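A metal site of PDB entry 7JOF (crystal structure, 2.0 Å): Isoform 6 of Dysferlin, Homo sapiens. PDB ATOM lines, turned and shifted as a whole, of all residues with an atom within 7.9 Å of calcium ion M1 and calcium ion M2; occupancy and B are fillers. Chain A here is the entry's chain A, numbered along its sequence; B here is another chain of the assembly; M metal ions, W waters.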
ATOM      1  N   THR A  20     -12.684 -12.491  20.998  1.00  0.00           N
ATOM      2  CA  THR A  20     -13.302 -12.590  19.652  1.00  0.00           C
ATOM      3  C   THR A  20     -14.402 -11.546  19.503  1.00  0.00           C
ATOM      4  O   THR A  20     -14.840 -10.963  20.488  1.00  0.00           O
ATOM      5  CB  THR A  20     -14.003 -13.928  19.389  1.00  0.00           C
ATOM      6  OG1 THR A  20     -15.252 -14.038  20.061  1.00  0.00           O
ATOM      7  CG2 THR A  20     -13.147 -15.105  19.748  1.00  0.00           C
ATOM      8  N   ASP A  22     -17.572 -12.017  19.338  1.00  0.00           N
ATOM      9  CA  ASP A  22     -18.934 -12.413  19.806  1.00  0.00           C
ATOM     10  C   ASP A  22     -18.829 -13.277  21.067  1.00  0.00           C
ATOM     11  O   ASP A  22     -17.862 -13.178  21.751  1.00  0.00           O
ATOM     12  CB  ASP A  22     -19.771 -13.104  18.729  1.00  0.00           C
ATOM     13  CG  ASP A  22     -19.012 -14.190  18.000  1.00  0.00           C
ATOM     14  OD1 ASP A  22     -18.173 -14.784  18.608  1.00  0.00           O
ATOM     15  OD2 ASP A  22     -19.291 -14.379  16.854  1.00  0.00           O
ATOM     16  N   THR A  23     -19.803 -14.170  21.280  1.00  0.00           N
ATOM     17  CA  THR A  23     -19.894 -15.050  22.478  1.00  0.00           C
ATOM     18  C   THR A  23     -18.858 -16.191  22.449  1.00  0.00           C
ATOM     19  O   THR A  23     -18.633 -16.777  23.481  1.00  0.00           O
ATOM     20  CB  THR A  23     -21.325 -15.546  22.683  1.00  0.00           C
ATOM     21  OG1 THR A  23     -21.610 -16.371  21.555  1.00  0.00           O
ATOM     22  CG2 THR A  23     -22.337 -14.422  22.865  1.00  0.00           C
ATOM     23  N   ASP A  24     -18.282 -16.466  21.280  1.00  0.00           N
ATOM     24  CA  ASP A  24     -17.264 -17.541  21.108  1.00  0.00           C
ATOM     25  C   ASP A  24     -16.018 -17.193  21.917  1.00  0.00           C
ATOM     26  O   ASP A  24     -15.622 -16.003  21.918  1.00  0.00           O
ATOM     27  CB  ASP A  24     -16.950 -17.783  19.638  1.00  0.00           C
ATOM     28  CG  ASP A  24     -15.801 -18.751  19.424  1.00  0.00           C
ATOM     29  OD1 ASP A  24     -15.873 -19.875  19.964  1.00  0.00           O
ATOM     30  OD2 ASP A  24     -14.843 -18.378  18.713  1.00  0.00           O
ATOM     31  N   ILE A  25     -15.423 -18.187  22.581  1.00  0.00           N
ATOM     32  CA  ILE A  25     -14.198 -17.993  23.402  1.00  0.00           C
ATOM     33  C   ILE A  25     -13.046 -18.161  22.416  1.00  0.00           C
ATOM     34  O   ILE A  25     -13.026 -19.169  21.794  1.00  0.00           O
ATOM     35  CB  ILE A  25     -14.152 -19.015  24.541  1.00  0.00           C
ATOM     36  CG1 ILE A  25     -15.417 -18.968  25.419  1.00  0.00           C
ATOM     37  CG2 ILE A  25     -12.897 -18.823  25.360  1.00  0.00           C
ATOM     38  CD1 ILE A  25     -15.900 -17.596  25.702  1.00  0.00           C
ATOM     39  N   SER A  26     -12.184 -17.155  22.272  1.00  0.00           N
ATOM     40  CA  SER A  26     -11.019 -17.159  21.333  1.00  0.00           C
ATOM     41  C   SER A  26     -10.368 -18.542  21.107  1.00  0.00           C
ATOM     42  O   SER A  26     -10.014 -19.226  22.064  1.00  0.00           O
ATOM     43  CB  SER A  26      -9.992 -16.110  21.719  1.00  0.00           C
ATOM     44  OG  SER A  26     -10.527 -14.804  21.700  1.00  0.00           O
ATOM     45  N   ASP A  27     -10.230 -18.897  19.843  1.00  0.00           N
ATOM     46  CA  ASP A  27      -9.487 -20.107  19.406  1.00  0.00           C
ATOM     47  C   ASP A  27      -8.281 -19.523  18.690  1.00  0.00           C
ATOM     48  O   ASP A  27      -8.246 -19.477  17.463  1.00  0.00           O
ATOM     49  CB  ASP A  27     -10.349 -21.015  18.560  1.00  0.00           C
ATOM     50  CG  ASP A  27     -11.665 -21.299  19.222  1.00  0.00           C
ATOM     51  OD1 ASP A  27     -11.659 -21.955  20.270  1.00  0.00           O
ATOM     52  OD2 ASP A  27     -12.636 -20.839  18.709  1.00  0.00           O
ATOM     53  N   ALA A  28      -7.382 -19.027  19.523  1.00  0.00           N
ATOM     54  CA  ALA A  28      -6.287 -18.191  19.024  1.00  0.00           C
ATOM     55  C   ALA A  28      -5.081 -18.965  18.537  1.00  0.00           C
ATOM     56  O   ALA A  28      -4.732 -19.990  19.104  1.00  0.00           O
ATOM     57  CB  ALA A  28      -5.883 -17.162  20.051  1.00  0.00           C
ATOM     58  N   VAL A  43      -3.576 -23.935  17.255  1.00  0.00           N
ATOM     59  CA  VAL A  43      -4.776 -23.251  17.790  1.00  0.00           C
ATOM     60  C   VAL A  43      -4.966 -23.644  19.261  1.00  0.00           C
ATOM     61  O   VAL A  43      -4.917 -24.838  19.568  1.00  0.00           O
ATOM     62  CB  VAL A  43      -6.019 -23.657  16.963  1.00  0.00           C
ATOM     63  CG1 VAL A  43      -7.328 -23.188  17.530  1.00  0.00           C
ATOM     64  CG2 VAL A  43      -5.912 -23.268  15.502  1.00  0.00           C
ATOM     65  N   ILE A  44      -5.045 -22.667  20.148  1.00  0.00           N
ATOM     66  CA  ILE A  44      -5.394 -22.999  21.563  1.00  0.00           C
ATOM     67  C   ILE A  44      -6.924 -22.902  21.641  1.00  0.00           C
ATOM     68  O   ILE A  44      -7.434 -21.811  21.566  1.00  0.00           O
ATOM     69  CB  ILE A  44      -4.716 -22.078  22.596  1.00  0.00           C
ATOM     70  CG1 ILE A  44      -3.188 -22.208  22.602  1.00  0.00           C
ATOM     71  CG2 ILE A  44      -5.334 -22.354  23.955  1.00  0.00           C
ATOM     72  CD1 ILE A  44      -2.686 -23.561  22.282  1.00  0.00           C
ATOM     73  N   LYS A  45      -7.605 -24.014  21.756  1.00  0.00           N
ATOM     74  CA  LYS A  45      -9.092 -23.983  21.807  1.00  0.00           C
ATOM     75  C   LYS A  45      -9.597 -23.281  23.080  1.00  0.00           C
ATOM     76  O   LYS A  45      -9.069 -23.550  24.158  1.00  0.00           O
ATOM     77  CB  LYS A  45      -9.671 -25.401  21.788  1.00  0.00           C
ATOM     78  CG  LYS A  45      -8.951 -26.393  20.888  1.00  0.00           C
ATOM     79  CD  LYS A  45      -9.506 -27.793  20.999  1.00  0.00           C
ATOM     80  CE  LYS A  45      -8.821 -28.771  20.068  1.00  0.00           C
ATOM     81  NZ  LYS A  45      -9.811 -29.545  19.275  1.00  0.00           N
ATOM     82  N   ASN A  46     -10.588 -22.418  22.916  1.00  0.00           N
ATOM     83  CA  ASN A  46     -11.345 -21.819  24.052  1.00  0.00           C
ATOM     84  C   ASN A  46     -10.452 -21.173  25.136  1.00  0.00           C
ATOM     85  O   ASN A  46     -10.528 -21.603  26.266  1.00  0.00           O
ATOM     86  CB  ASN A  46     -12.247 -22.906  24.656  1.00  0.00           C
ATOM     87  CG  ASN A  46     -13.342 -23.301  23.692  1.00  0.00           C
ATOM     88  OD1 ASN A  46     -13.842 -22.445  23.019  1.00  0.00           O
ATOM     89  ND2 ASN A  46     -13.740 -24.549  23.642  1.00  0.00           N
ATOM     90  N   SER A  47      -9.653 -20.194  24.768  1.00  0.00           N
ATOM     91  CA  SER A  47      -8.870 -19.441  25.755  1.00  0.00           C
ATOM     92  C   SER A  47      -8.664 -17.991  25.340  1.00  0.00           C
ATOM     93  O   SER A  47      -8.143 -17.743  24.287  1.00  0.00           O
ATOM     94  CB  SER A  47      -7.588 -20.122  26.155  1.00  0.00           C
ATOM     95  OG  SER A  47      -6.752 -19.227  26.798  1.00  0.00           O
ATOM     96  N   LYS A  76      -5.146 -14.636  14.908  1.00  0.00           N
ATOM     97  CA  LYS A  76      -6.456 -14.968  14.308  1.00  0.00           C
ATOM     98  C   LYS A  76      -7.267 -15.934  15.180  1.00  0.00           C
ATOM     99  O   LYS A  76      -6.676 -16.705  15.956  1.00  0.00           O
ATOM    100  CB  LYS A  76      -6.293 -15.534  12.905  1.00  0.00           C
ATOM    101  CG  LYS A  76      -5.743 -14.543  11.889  1.00  0.00           C
ATOM    102  CD  LYS A  76      -5.994 -14.870  10.467  1.00  0.00           C
ATOM    103  CE  LYS A  76      -4.795 -15.350   9.684  1.00  0.00           C
ATOM    104  NZ  LYS A  76      -5.173 -15.840   8.338  1.00  0.00           N
ATOM    105  N   ASP A  77      -8.578 -15.888  15.019  1.00  0.00           N
ATOM    106  CA  ASP A  77      -9.490 -16.801  15.726  1.00  0.00           C
ATOM    107  C   ASP A  77      -9.909 -17.919  14.772  1.00  0.00           C
ATOM    108  O   ASP A  77     -10.583 -17.642  13.798  1.00  0.00           O
ATOM    109  CB  ASP A  77     -10.682 -16.100  16.345  1.00  0.00           C
ATOM    110  CG  ASP A  77     -11.746 -17.127  16.716  1.00  0.00           C
ATOM    111  OD1 ASP A  77     -11.450 -18.021  17.512  1.00  0.00           O
ATOM    112  OD2 ASP A  77     -12.828 -17.019  16.147  1.00  0.00           O
ATOM    113  N   HIS A  78      -9.440 -19.121  15.069  1.00  0.00           N
ATOM    114  CA  HIS A  78      -9.828 -20.346  14.314  1.00  0.00           C
ATOM    115  C   HIS A  78     -11.373 -20.424  14.220  1.00  0.00           C
ATOM    116  O   HIS A  78     -11.992 -20.359  15.232  1.00  0.00           O
ATOM    117  CB  HIS A  78      -9.320 -21.597  15.029  1.00  0.00           C
ATOM    118  CG  HIS A  78      -9.762 -22.819  14.311  1.00  0.00           C
ATOM    119  ND1 HIS A  78     -10.862 -23.533  14.678  1.00  0.00           N
ATOM    120  CD2 HIS A  78      -9.308 -23.400  13.186  1.00  0.00           C
ATOM    121  CE1 HIS A  78     -11.004 -24.543  13.846  1.00  0.00           C
ATOM    122  NE2 HIS A  78     -10.082 -24.480  12.942  1.00  0.00           N
ATOM    123  N   GLU A  79     -11.926 -20.598  13.031  1.00  0.00           N
ATOM    124  CA  GLU A  79     -13.414 -20.655  12.972  1.00  0.00           C
ATOM    125  C   GLU A  79     -13.867 -22.083  12.624  1.00  0.00           C
ATOM    126  O   GLU A  79     -13.639 -22.493  11.512  1.00  0.00           O
ATOM    127  CB  GLU A  79     -13.838 -19.550  12.017  1.00  0.00           C
ATOM    128  CG  GLU A  79     -15.274 -19.142  12.158  1.00  0.00           C
ATOM    129  CD  GLU A  79     -15.735 -18.652  13.515  1.00  0.00           C
ATOM    130  OE1 GLU A  79     -14.935 -18.616  14.456  1.00  0.00           O
ATOM    131  OE2 GLU A  79     -16.890 -18.347  13.612  1.00  0.00           O
ATOM    132  N   THR A  80     -14.528 -22.769  13.565  1.00  0.00           N
ATOM    133  CA  THR A  80     -14.969 -24.207  13.522  1.00  0.00           C
ATOM    134  C   THR A  80     -15.454 -24.589  12.122  1.00  0.00           C
ATOM    135  O   THR A  80     -16.677 -24.465  11.857  1.00  0.00           O
ATOM    136  CB  THR A  80     -15.955 -24.549  14.660  1.00  0.00           C
ATOM    137  OG1 THR A  80     -16.123 -23.469  15.561  1.00  0.00           O
ATOM    138  CG2 THR A  80     -15.598 -25.793  15.447  1.00  0.00           C
ATOM    139  N   MET A  81     -14.477 -24.958  11.274  1.00  0.00           N
ATOM    140  CA  MET A  81     -14.576 -25.339   9.854  1.00  0.00           C
ATOM    141  C   MET A  81     -14.959 -24.126   8.999  1.00  0.00           C
ATOM    142  O   MET A  81     -16.142 -23.986   8.620  1.00  0.00           O
ATOM    143  CB  MET A  81     -15.547 -26.503   9.654  1.00  0.00           C
ATOM    144  CG  MET A  81     -14.895 -27.776   9.143  1.00  0.00           C
ATOM    145  SD  MET A  81     -15.739 -28.347   7.644  1.00  0.00           S
ATOM    146  CE  MET A  81     -16.937 -27.034   7.393  1.00  0.00           C
ATOM    147  N   ARG A  83     -13.259 -19.955   7.329  1.00  0.00           N
ATOM    148  CA  ARG A  83     -12.237 -18.889   7.225  1.00  0.00           C
ATOM    149  C   ARG A  83     -12.089 -18.242   8.594  1.00  0.00           C
ATOM    150  O   ARG A  83     -13.063 -17.770   9.169  1.00  0.00           O
ATOM    151  CB  ARG A  83     -12.547 -17.952   6.050  1.00  0.00           C
ATOM    152  CG  ARG A  83     -11.449 -16.946   5.742  1.00  0.00           C
ATOM    153  CD  ARG A  83     -10.799 -17.229   4.407  1.00  0.00           C
ATOM    154  NE  ARG A  83     -10.085 -16.092   3.853  1.00  0.00           N
ATOM    155  CZ  ARG A  83     -10.435 -15.462   2.744  1.00  0.00           C
ATOM    156  NH1 ARG A  83      -9.594 -15.394   1.735  1.00  0.00           N
ATOM    157  NH2 ARG A  83     -11.637 -14.916   2.631  1.00  0.00           N
ATOM    158  N   ASN A  84     -10.853 -18.259   9.086  1.00  0.00           N
ATOM    159  CA  ASN A  84     -10.467 -17.714  10.410  1.00  0.00           C
ATOM    160  C   ASN A  84     -10.682 -16.205  10.417  1.00  0.00           C
ATOM    161  O   ASN A  84     -10.554 -15.583   9.355  1.00  0.00           O
ATOM    162  CB  ASN A  84      -9.105 -18.284  10.796  1.00  0.00           C
ATOM    163  CG  ASN A  84      -9.056 -19.758  10.431  1.00  0.00           C
ATOM    164  OD1 ASN A  84     -10.044 -20.470  10.548  1.00  0.00           O
ATOM    165  ND2 ASN A  84      -7.879 -20.229  10.077  1.00  0.00           N
ATOM    166  N   ARG A  85     -10.943 -15.629  11.585  1.00  0.00           N
ATOM    167  CA  ARG A  85     -11.200 -14.179  11.718  1.00  0.00           C
ATOM    168  C   ARG A  85     -10.051 -13.462  12.433  1.00  0.00           C
ATOM    169  O   ARG A  85      -9.513 -13.962  13.401  1.00  0.00           O
ATOM    170  CB  ARG A  85     -12.572 -13.924  12.361  1.00  0.00           C
ATOM    171  CG  ARG A  85     -12.977 -14.977  13.378  1.00  0.00           C
ATOM    172  CD  ARG A  85     -14.440 -15.013  13.740  1.00  0.00           C
ATOM    173  NE  ARG A  85     -14.645 -15.145  15.153  1.00  0.00           N
ATOM    174  CZ  ARG A  85     -15.832 -15.125  15.743  1.00  0.00           C
ATOM    175  NH1 ARG A  85     -16.735 -14.206  15.455  1.00  0.00           N
ATOM    176  NH2 ARG A  85     -16.072 -16.032  16.653  1.00  0.00           N
ATOM    177  N   LEU A  87      -8.048 -11.066  14.764  1.00  0.00           N
ATOM    178  CA  LEU A  87      -8.270 -10.625  16.157  1.00  0.00           C
ATOM    179  C   LEU A  87      -7.389  -9.399  16.422  1.00  0.00           C
ATOM    180  O   LEU A  87      -7.834  -8.507  16.976  1.00  0.00           O
ATOM    181  CB  LEU A  87      -7.962 -11.761  17.133  1.00  0.00           C
ATOM    182  CG  LEU A  87      -8.956 -12.921  17.207  1.00  0.00           C
ATOM    183  CD1 LEU A  87      -8.701 -13.784  18.426  1.00  0.00           C
ATOM    184  CD2 LEU A  87     -10.385 -12.442  17.139  1.00  0.00           C
ATOM    185  N   THR B 114     -21.923 -16.011  15.447  1.00  0.00           N
ATOM    186  CA  THR B 114     -21.392 -17.282  14.893  1.00  0.00           C
ATOM    187  C   THR B 114     -21.784 -18.453  15.795  1.00  0.00           C
ATOM    188  O   THR B 114     -21.690 -19.599  15.323  1.00  0.00           O
ATOM    189  CB  THR B 114     -19.868 -17.206  14.712  1.00  0.00           C
ATOM    190  OG1 THR B 114     -19.291 -16.903  15.985  1.00  0.00           O
ATOM    191  CG2 THR B 114     -19.440 -16.175  13.692  1.00  0.00           C
ATOM    192  N   LYS B 115     -22.183 -18.188  17.043  1.00  0.00           N
ATOM    193  CA  LYS B 115     -22.539 -19.252  18.012  1.00  0.00           C
ATOM    194  C   LYS B 115     -24.051 -19.283  18.257  1.00  0.00           C
ATOM    195  O   LYS B 115     -24.485 -19.934  19.227  1.00  0.00           O
ATOM    196  CB  LYS B 115     -21.770 -19.067  19.322  1.00  0.00           C
ATOM    197  CG  LYS B 115     -20.302 -19.445  19.282  1.00  0.00           C
ATOM    198  CD  LYS B 115     -20.069 -20.919  19.050  1.00  0.00           C
ATOM    199  CE  LYS B 115     -18.634 -21.348  19.314  1.00  0.00           C
ATOM    200  NZ  LYS B 115     -17.892 -21.569  18.053  1.00  0.00           N
HETATM  201 CA    CA M   1     -13.614 -19.483  16.743  1.00  0.00          CA
HETATM  202 CA    CA M   2     -14.232 -21.261  20.764  1.00  0.00          CA
HETATM  203  O   HOH W   1     -15.288 -21.341  16.830  1.00  0.00           O
HETATM  204  O   HOH W   2     -15.659 -23.005  19.389  1.00  0.00           O
HETATM  205  O   HOH W   3     -16.238 -20.973  22.499  1.00  0.00           O
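Calcium ion M1 is bound by the backbone carbonyl oxygen (O) of His 78. Water W1 binds calcium ion M1 (2.5 Å). Calcium ion M1 is bound by OD2 of Asp 24 (2.6 Å). The side-chain carboxylate (OD2) of Asp 27 is bound to calcium ion M1, 2.6 Å away. OD2 of Asp 77 is bound to calcium ion M1, 2.7 Å away. OD1 of Asp 77 binds calcium ion M1, 2.7 Å away. The side-chain carboxylate (OE1) of Glu 79 is bound to calcium ion M1 (2.8 Å).
Water W1 lies within hydrogen-bond range of OG1 of Thr 80 (2.6 Å) and NZ of Lys 115 of chain B (2.9 Å).
Within 4 Å of calcium ion M2: Asp 24, Ile 25, Asp 27 and Asn 46. The nearest printed residue that does not touch calcium ion M2 is Lys 115 of chain B (4.6 Å).
Calcium ion M2 is bound by OD1 of Asp 24, OD1 of Asn 46, O of Ile 25, OD2 of Asp 27, water W2, water W3 and OD1 of Asp 27. Calcium ion M2 has seven donor atoms within binding distance.
Of the 25 residues printed, 5 come within 4 Å of calcium ion M1. The nearest printed residue that does not touch calcium ion M1 is Arg 85 (4.2 Å).
N of Asp 77 is in hydrogen-bond range of O of Arg 85 (2.7 Å). OE2 of Glu 79 lies within salt-bridge range of NH2 of Arg 85 (3.9 Å). N of Glu 79 sits at hydrogen-bond distance from OD1 of Asn 84 (3.1 Å). The side-chain amino group of Lys 115 of chain B lies close to the side-chain carboxylate of Asp 24, 3.3 Å away. The side-chain carboxylate of Asp 24 sits close to the guanidinium group of Arg 85. The side-chain carboxylate of Asp 22 sits at hydrogen-bond distance from the backbone NH of Asp 24 (3.2 Å). OG1 of Thr 20 is in hydrogen-bond range of O of Asp 24 (2.7 Å). O of Ser 26 is in hydrogen-bond range of N of Asn 46, at 3.4 Å.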
